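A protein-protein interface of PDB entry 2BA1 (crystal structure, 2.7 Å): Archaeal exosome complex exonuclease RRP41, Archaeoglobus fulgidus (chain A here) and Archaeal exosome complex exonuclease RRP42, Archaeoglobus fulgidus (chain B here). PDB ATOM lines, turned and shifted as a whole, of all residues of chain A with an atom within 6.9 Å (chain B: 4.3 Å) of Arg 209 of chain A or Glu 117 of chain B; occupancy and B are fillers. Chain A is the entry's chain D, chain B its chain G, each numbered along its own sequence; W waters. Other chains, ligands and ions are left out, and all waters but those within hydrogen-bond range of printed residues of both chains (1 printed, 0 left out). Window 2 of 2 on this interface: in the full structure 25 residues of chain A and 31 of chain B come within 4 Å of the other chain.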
ATOM      1  N   LYS A 166     -11.685 -36.748  -1.864  1.00  0.00           N
ATOM      2  CA  LYS A 166     -10.835 -36.949  -0.710  1.00  0.00           C
ATOM      3  C   LYS A 166     -11.718 -36.773   0.509  1.00  0.00           C
ATOM      4  O   LYS A 166     -12.304 -35.709   0.713  1.00  0.00           O
ATOM      5  CB  LYS A 166      -9.701 -35.928  -0.691  1.00  0.00           C
ATOM      6  CG  LYS A 166      -8.783 -36.047   0.519  1.00  0.00           C
ATOM      7  CD  LYS A 166      -7.652 -35.038   0.426  1.00  0.00           C
ATOM      8  CE  LYS A 166      -6.746 -35.100   1.634  1.00  0.00           C
ATOM      9  NZ  LYS A 166      -5.610 -34.165   1.453  1.00  0.00           N
ATOM     10  N   GLU A 184     -12.216 -33.025   1.475  1.00  0.00           N
ATOM     11  CA  GLU A 184     -11.143 -32.050   1.337  1.00  0.00           C
ATOM     12  C   GLU A 184     -10.802 -31.716  -0.106  1.00  0.00           C
ATOM     13  O   GLU A 184     -10.050 -30.778  -0.364  1.00  0.00           O
ATOM     14  CB  GLU A 184      -9.874 -32.540   2.043  1.00  0.00           C
ATOM     15  CG  GLU A 184      -9.985 -32.640   3.553  1.00  0.00           C
ATOM     16  CD  GLU A 184     -10.335 -34.037   4.014  1.00  0.00           C
ATOM     17  OE1 GLU A 184      -9.546 -34.965   3.719  1.00  0.00           O
ATOM     18  OE2 GLU A 184     -11.392 -34.203   4.667  1.00  0.00           O
ATOM     19  N   ALA A 185     -11.345 -32.482  -1.046  1.00  0.00           N
ATOM     20  CA  ALA A 185     -11.061 -32.243  -2.453  1.00  0.00           C
ATOM     21  C   ALA A 185     -12.073 -32.917  -3.372  1.00  0.00           C
ATOM     22  O   ALA A 185     -12.808 -33.812  -2.960  1.00  0.00           O
ATOM     23  CB  ALA A 185      -9.645 -32.726  -2.784  1.00  0.00           C
ATOM     24  N   ASP A 186     -12.095 -32.474  -4.624  1.00  0.00           N
ATOM     25  CA  ASP A 186     -13.000 -32.999  -5.640  1.00  0.00           C
ATOM     26  C   ASP A 186     -12.241 -32.842  -6.957  1.00  0.00           C
ATOM     27  O   ASP A 186     -11.833 -31.736  -7.302  1.00  0.00           O
ATOM     28  CB  ASP A 186     -14.287 -32.160  -5.670  1.00  0.00           C
ATOM     29  CG  ASP A 186     -14.642 -31.573  -4.296  1.00  0.00           C
ATOM     30  OD1 ASP A 186     -14.874 -32.365  -3.354  1.00  0.00           O
ATOM     31  OD2 ASP A 186     -14.686 -30.324  -4.148  1.00  0.00           O
ATOM     32  N   MET A 206      -9.547 -29.560 -10.615  1.00  0.00           N
ATOM     33  CA  MET A 206      -9.443 -29.906  -9.196  1.00  0.00           C
ATOM     34  C   MET A 206      -9.816 -28.756  -8.266  1.00  0.00           C
ATOM     35  O   MET A 206      -9.579 -27.594  -8.564  1.00  0.00           O
ATOM     36  CB  MET A 206      -8.029 -30.424  -8.860  1.00  0.00           C
ATOM     37  CG  MET A 206      -7.108 -29.487  -8.046  1.00  0.00           C
ATOM     38  SD  MET A 206      -7.447 -29.328  -6.242  1.00  0.00           S
ATOM     39  CE  MET A 206      -6.449 -30.595  -5.598  1.00  0.00           C
ATOM     40  N   ASP A 207     -10.411 -29.099  -7.135  1.00  0.00           N
ATOM     41  CA  ASP A 207     -10.801 -28.125  -6.121  1.00  0.00           C
ATOM     42  C   ASP A 207     -10.538 -28.761  -4.766  1.00  0.00           C
ATOM     43  O   ASP A 207     -10.755 -29.959  -4.582  1.00  0.00           O
ATOM     44  CB  ASP A 207     -12.291 -27.774  -6.225  1.00  0.00           C
ATOM     45  CG  ASP A 207     -12.585 -26.768  -7.324  1.00  0.00           C
ATOM     46  OD1 ASP A 207     -12.092 -25.624  -7.231  1.00  0.00           O
ATOM     47  OD2 ASP A 207     -13.315 -27.118  -8.279  1.00  0.00           O
ATOM     48  N   GLY A 208     -10.071 -27.961  -3.818  1.00  0.00           N
ATOM     49  CA  GLY A 208      -9.795 -28.484  -2.492  1.00  0.00           C
ATOM     50  C   GLY A 208      -8.374 -28.210  -2.058  1.00  0.00           C
ATOM     51  O   GLY A 208      -7.881 -27.089  -2.180  1.00  0.00           O
ATOM     52  N   ARG A 209      -7.707 -29.241  -1.560  1.00  0.00           N
ATOM     53  CA  ARG A 209      -6.335 -29.110  -1.093  1.00  0.00           C
ATOM     54  C   ARG A 209      -5.665 -30.476  -1.123  1.00  0.00           C
ATOM     55  O   ARG A 209      -5.989 -31.353  -0.326  1.00  0.00           O
ATOM     56  CB  ARG A 209      -6.330 -28.544   0.330  1.00  0.00           C
ATOM     57  CG  ARG A 209      -4.952 -28.356   0.933  1.00  0.00           C
ATOM     58  CD  ARG A 209      -5.049 -27.833   2.356  1.00  0.00           C
ATOM     59  NE  ARG A 209      -5.402 -26.415   2.402  1.00  0.00           N
ATOM     60  CZ  ARG A 209      -6.449 -25.920   3.061  1.00  0.00           C
ATOM     61  NH1 ARG A 209      -6.679 -24.614   3.046  1.00  0.00           N
ATOM     62  NH2 ARG A 209      -7.270 -26.725   3.726  1.00  0.00           N
ATOM     63  N   MET A 210      -4.733 -30.649  -2.049  1.00  0.00           N
ATOM     64  CA  MET A 210      -4.036 -31.913  -2.199  1.00  0.00           C
ATOM     65  C   MET A 210      -2.528 -31.741  -2.340  1.00  0.00           C
ATOM     66  O   MET A 210      -2.048 -30.740  -2.875  1.00  0.00           O
ATOM     67  CB  MET A 210      -4.551 -32.646  -3.431  1.00  0.00           C
ATOM     68  CG  MET A 210      -5.969 -33.123  -3.333  1.00  0.00           C
ATOM     69  SD  MET A 210      -6.471 -33.884  -4.879  1.00  0.00           S
ATOM     70  CE  MET A 210      -5.653 -35.460  -4.783  1.00  0.00           C
ATOM     71  N   THR A 211      -1.786 -32.741  -1.874  1.00  0.00           N
ATOM     72  CA  THR A 211      -0.334 -32.720  -1.962  1.00  0.00           C
ATOM     73  C   THR A 211       0.081 -33.160  -3.363  1.00  0.00           C
ATOM     74  O   THR A 211      -0.727 -33.678  -4.123  1.00  0.00           O
ATOM     75  CB  THR A 211       0.297 -33.673  -0.930  1.00  0.00           C
ATOM     76  OG1 THR A 211      -0.175 -35.007  -1.164  1.00  0.00           O
ATOM     77  CG2 THR A 211      -0.071 -33.244   0.483  1.00  0.00           C
ATOM     78  N   GLU A 214      -0.607 -37.026  -3.633  1.00  0.00           N
ATOM     79  CA  GLU A 214      -2.039 -37.289  -3.714  1.00  0.00           C
ATOM     80  C   GLU A 214      -2.601 -37.046  -5.113  1.00  0.00           C
ATOM     81  O   GLU A 214      -3.355 -37.866  -5.638  1.00  0.00           O
ATOM     82  CB  GLU A 214      -2.790 -36.420  -2.707  1.00  0.00           C
ATOM     83  CG  GLU A 214      -2.580 -36.839  -1.272  1.00  0.00           C
ATOM     84  CD  GLU A 214      -3.505 -36.121  -0.310  1.00  0.00           C
ATOM     85  OE1 GLU A 214      -3.259 -34.932  -0.005  1.00  0.00           O
ATOM     86  OE2 GLU A 214      -4.487 -36.754   0.133  1.00  0.00           O
ATOM     87  N   ILE B 113      -8.579 -18.727  -4.275  1.00  0.00           N
ATOM     88  CA  ILE B 113      -8.842 -17.972  -3.057  1.00  0.00           C
ATOM     89  C   ILE B 113      -9.684 -18.785  -2.072  1.00  0.00           C
ATOM     90  O   ILE B 113      -9.374 -18.856  -0.887  1.00  0.00           O
ATOM     91  CB  ILE B 113      -9.618 -16.667  -3.360  1.00  0.00           C
ATOM     92  CG1 ILE B 113      -8.825 -15.778  -4.313  1.00  0.00           C
ATOM     93  CG2 ILE B 113      -9.910 -15.926  -2.073  1.00  0.00           C
ATOM     94  CD1 ILE B 113      -7.623 -15.172  -3.698  1.00  0.00           C
ATOM     95  N   ARG B 114     -10.754 -19.394  -2.566  1.00  0.00           N
ATOM     96  CA  ARG B 114     -11.643 -20.174  -1.711  1.00  0.00           C
ATOM     97  C   ARG B 114     -11.059 -21.489  -1.192  1.00  0.00           C
ATOM     98  O   ARG B 114     -11.129 -21.767   0.005  1.00  0.00           O
ATOM     99  CB  ARG B 114     -12.971 -20.439  -2.439  1.00  0.00           C
ATOM    100  CG  ARG B 114     -13.947 -21.317  -1.661  1.00  0.00           C
ATOM    101  CD  ARG B 114     -15.360 -21.341  -2.273  1.00  0.00           C
ATOM    102  NE  ARG B 114     -16.126 -20.129  -1.964  1.00  0.00           N
ATOM    103  CZ  ARG B 114     -16.263 -19.090  -2.783  1.00  0.00           C
ATOM    104  NH1 ARG B 114     -16.970 -18.036  -2.406  1.00  0.00           N
ATOM    105  NH2 ARG B 114     -15.706 -19.112  -3.986  1.00  0.00           N
ATOM    106  N   GLU B 115     -10.473 -22.290  -2.080  1.00  0.00           N
ATOM    107  CA  GLU B 115      -9.918 -23.573  -1.667  1.00  0.00           C
ATOM    108  C   GLU B 115      -8.668 -23.487  -0.799  1.00  0.00           C
ATOM    109  O   GLU B 115      -8.444 -24.352   0.049  1.00  0.00           O
ATOM    110  CB  GLU B 115      -9.642 -24.462  -2.883  1.00  0.00           C
ATOM    111  CG  GLU B 115     -10.877 -24.839  -3.713  1.00  0.00           C
ATOM    112  CD  GLU B 115     -12.046 -25.359  -2.869  1.00  0.00           C
ATOM    113  OE1 GLU B 115     -11.797 -26.105  -1.893  1.00  0.00           O
ATOM    114  OE2 GLU B 115     -13.215 -25.036  -3.193  1.00  0.00           O
ATOM    115  N   SER B 116      -7.852 -22.455  -0.994  1.00  0.00           N
ATOM    116  CA  SER B 116      -6.640 -22.297  -0.185  1.00  0.00           C
ATOM    117  C   SER B 116      -7.020 -21.699   1.171  1.00  0.00           C
ATOM    118  O   SER B 116      -6.214 -21.685   2.101  1.00  0.00           O
ATOM    119  CB  SER B 116      -5.644 -21.365  -0.875  1.00  0.00           C
ATOM    120  OG  SER B 116      -6.078 -20.019  -0.783  1.00  0.00           O
ATOM    121  N   GLU B 117      -8.257 -21.212   1.262  1.00  0.00           N
ATOM    122  CA  GLU B 117      -8.786 -20.587   2.471  1.00  0.00           C
ATOM    123  C   GLU B 117      -7.947 -19.390   2.886  1.00  0.00           C
ATOM    124  O   GLU B 117      -7.707 -19.164   4.075  1.00  0.00           O
ATOM    125  CB  GLU B 117      -8.859 -21.589   3.620  1.00  0.00           C
ATOM    126  CG  GLU B 117      -9.885 -22.677   3.413  1.00  0.00           C
ATOM    127  CD  GLU B 117     -10.161 -23.460   4.676  1.00  0.00           C
ATOM    128  OE1 GLU B 117     -10.231 -24.707   4.601  1.00  0.00           O
ATOM    129  N   ALA B 118      -7.506 -18.629   1.889  1.00  0.00           N
ATOM    130  CA  ALA B 118      -6.689 -17.446   2.110  1.00  0.00           C
ATOM    131  C   ALA B 118      -7.445 -16.392   2.913  1.00  0.00           C
ATOM    132  O   ALA B 118      -6.841 -15.472   3.455  1.00  0.00           O
ATOM    133  CB  ALA B 118      -6.233 -16.869   0.773  1.00  0.00           C
ATOM    134  N   VAL B 119      -8.765 -16.524   2.988  1.00  0.00           N
ATOM    135  CA  VAL B 119      -9.563 -15.576   3.754  1.00  0.00           C
ATOM    136  C   VAL B 119     -10.460 -16.319   4.736  1.00  0.00           C
ATOM    137  O   VAL B 119     -11.350 -17.064   4.333  1.00  0.00           O
ATOM    138  CB  VAL B 119     -10.441 -14.697   2.833  1.00  0.00           C
ATOM    139  CG1 VAL B 119     -11.221 -13.684   3.665  1.00  0.00           C
ATOM    140  CG2 VAL B 119      -9.569 -13.982   1.812  1.00  0.00           C
ATOM    141  N   ARG B 181      -4.714 -15.490   5.428  1.00  0.00           N
ATOM    142  CA  ARG B 181      -3.876 -16.571   5.955  1.00  0.00           C
ATOM    143  C   ARG B 181      -3.218 -17.510   4.943  1.00  0.00           C
ATOM    144  O   ARG B 181      -2.690 -18.550   5.325  1.00  0.00           O
ATOM    145  CB  ARG B 181      -4.666 -17.414   6.979  1.00  0.00           C
ATOM    146  CG  ARG B 181      -5.660 -18.396   6.379  1.00  0.00           C
ATOM    147  N   ASP B 217      -0.906 -23.390  -2.776  1.00  0.00           N
ATOM    148  CA  ASP B 217      -1.108 -22.548  -1.599  1.00  0.00           C
ATOM    149  C   ASP B 217       0.228 -22.222  -0.919  1.00  0.00           C
ATOM    150  O   ASP B 217       1.300 -22.419  -1.496  1.00  0.00           O
ATOM    151  CB  ASP B 217      -2.077 -23.224  -0.612  1.00  0.00           C
ATOM    152  CG  ASP B 217      -1.449 -24.381   0.146  1.00  0.00           C
ATOM    153  OD1 ASP B 217      -0.594 -25.094  -0.417  1.00  0.00           O
ATOM    154  OD2 ASP B 217      -1.834 -24.589   1.310  1.00  0.00           O
ATOM    155  N   ASN B 221       0.864 -26.952  -1.607  1.00  0.00           N
ATOM    156  CA  ASN B 221      -0.148 -27.953  -1.932  1.00  0.00           C
ATOM    157  C   ASN B 221      -0.994 -27.442  -3.090  1.00  0.00           C
ATOM    158  O   ASN B 221      -1.134 -26.230  -3.280  1.00  0.00           O
ATOM    159  CB  ASN B 221      -1.076 -28.216  -0.749  1.00  0.00           C
ATOM    160  CG  ASN B 221      -0.362 -28.834   0.427  1.00  0.00           C
ATOM    161  OD1 ASN B 221       0.538 -29.661   0.262  1.00  0.00           O
ATOM    162  ND2 ASN B 221      -0.768 -28.445   1.627  1.00  0.00           N
ATOM    163  N   VAL B 222      -1.552 -28.368  -3.865  1.00  0.00           N
ATOM    164  CA  VAL B 222      -2.399 -28.006  -4.991  1.00  0.00           C
ATOM    165  C   VAL B 222      -3.795 -27.716  -4.463  1.00  0.00           C
ATOM    166  O   VAL B 222      -4.469 -28.583  -3.892  1.00  0.00           O
ATOM    167  CB  VAL B 222      -2.464 -29.127  -6.028  1.00  0.00           C
ATOM    168  CG1 VAL B 222      -3.319 -28.692  -7.188  1.00  0.00           C
ATOM    169  CG2 VAL B 222      -1.061 -29.461  -6.509  1.00  0.00           C
HETATM  170  O   HOH W   1     -13.979 -23.688  -5.565  1.00  0.00           O
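Among the printed residues, pairs that only touch across the chains: Met 206 of chain A with Val 222 of chain B, Arg 209 of chain A with Val 222 of chain B, Met 210 of chain A with Asn 221 of chain B, Thr 211 of chain A with Asn 221 of chain B and Asp 207 of chain A with Glu 115 of chain B.
Printed residues of chain A that touch a printed residue of chain B: Met 206, Asp 207, Gly 208, Arg 209, Met 210 and Thr 211. Hydrophobic or aromatic side chains of chain A that line the printed part of chain B: Met 206. Printed residues of chain B that touch a printed residue of chain A: Glu 115, Ser 116, Glu 117, Asn 221 and Val 222. Hydrophobic or aromatic side chains of chain B that line the printed part of chain A: Val 222. Along chain B the printed residues that touch a printed residue of chain A span positions 115 to 222.
Water W1 lies within hydrogen-bond range of the side-chain carboxylate of Glu 115 of chain B (2.8 Å) and the side-chain carboxylate of Asp 207 of chain A (3.2 Å).
N of Glu 214 of chain A lies close to OG1 of Thr 211 of chain A, 3.2 Å away. N of Asn 221 of chain B lies within hydrogen-bond range of OD1 of Asp 217 of chain B, at 2.6 Å. The side-chain hydroxyl (OG) of Ser 116 of chain B sits close to the backbone NH (N) of Ala 118 of chain B (3.3 Å). The backbone carbonyl oxygen (O) of Ile 113 of chain B sits at hydrogen-bond distance from the side-chain hydroxyl (OG) of Ser 116 of chain B (3.5 Å). The backbone carbonyl oxygen (O) of Asp 207 of chain A lies within hydrogen-bond range of the backbone NH (N) of Asp 186 of chain A (2.9 Å). The side-chain amino group (NZ) of Lys 166 of chain A is in hydrogen-bond range of the backbone carbonyl oxygen (O) of Arg 209 of chain A, at 3.3 Å.
Asp 186 of chain A touches none of the printed residues of chain B. Of the printed residues of chain B, Gly 208 of chain A touches Glu 115. Arg 209 of chain A touches just these residues of chain B: Glu 115 (3.5 Å), Ser 116 (3.1 Å), Glu 117 (3.7 Å) and Val 222 (3.4 Å). Of the printed residues of chain A, Ser 116 of chain B touches Arg 209. Of chain A, only Arg 209 (3.7 Å) comes within 4 Å of Glu 117 of chain B. Arg 181 of chain B touches none of the printed residues of chain A. The nearest residue of chain B that does not touch Arg 209 of chain A is Asp 217 of chain B (4.2 Å). The nearest residue of chain A that does not touch Glu 117 of chain B is Gly 208 of chain A (6.8 Å). The nearest printed residue of chain B that does not touch Thr 211 of chain A is Val 222 of chain B (4.8 Å).
N of Gly 208 of chain A sits close to OE1 of Glu 115 of chain B (3.2 Å). NH1 of Arg 209 of chain A is in hydrogen-bond range of O of Glu 115 of chain B. N of Val 222 of chain B lies within hydrogen-bond range of O of Met 210 of chain A. The guanidinium group (NH1) of Arg 209 of chain A lies within hydrogen-bond range of the backbone carbonyl oxygen (O) of Ser 116 of chain B, at 3.1 Å. The side-chain carboxylate (OE1) of Glu 117 of chain B is in salt-bridge range of the guanidinium group (NH2) of Arg 209 of chain A.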
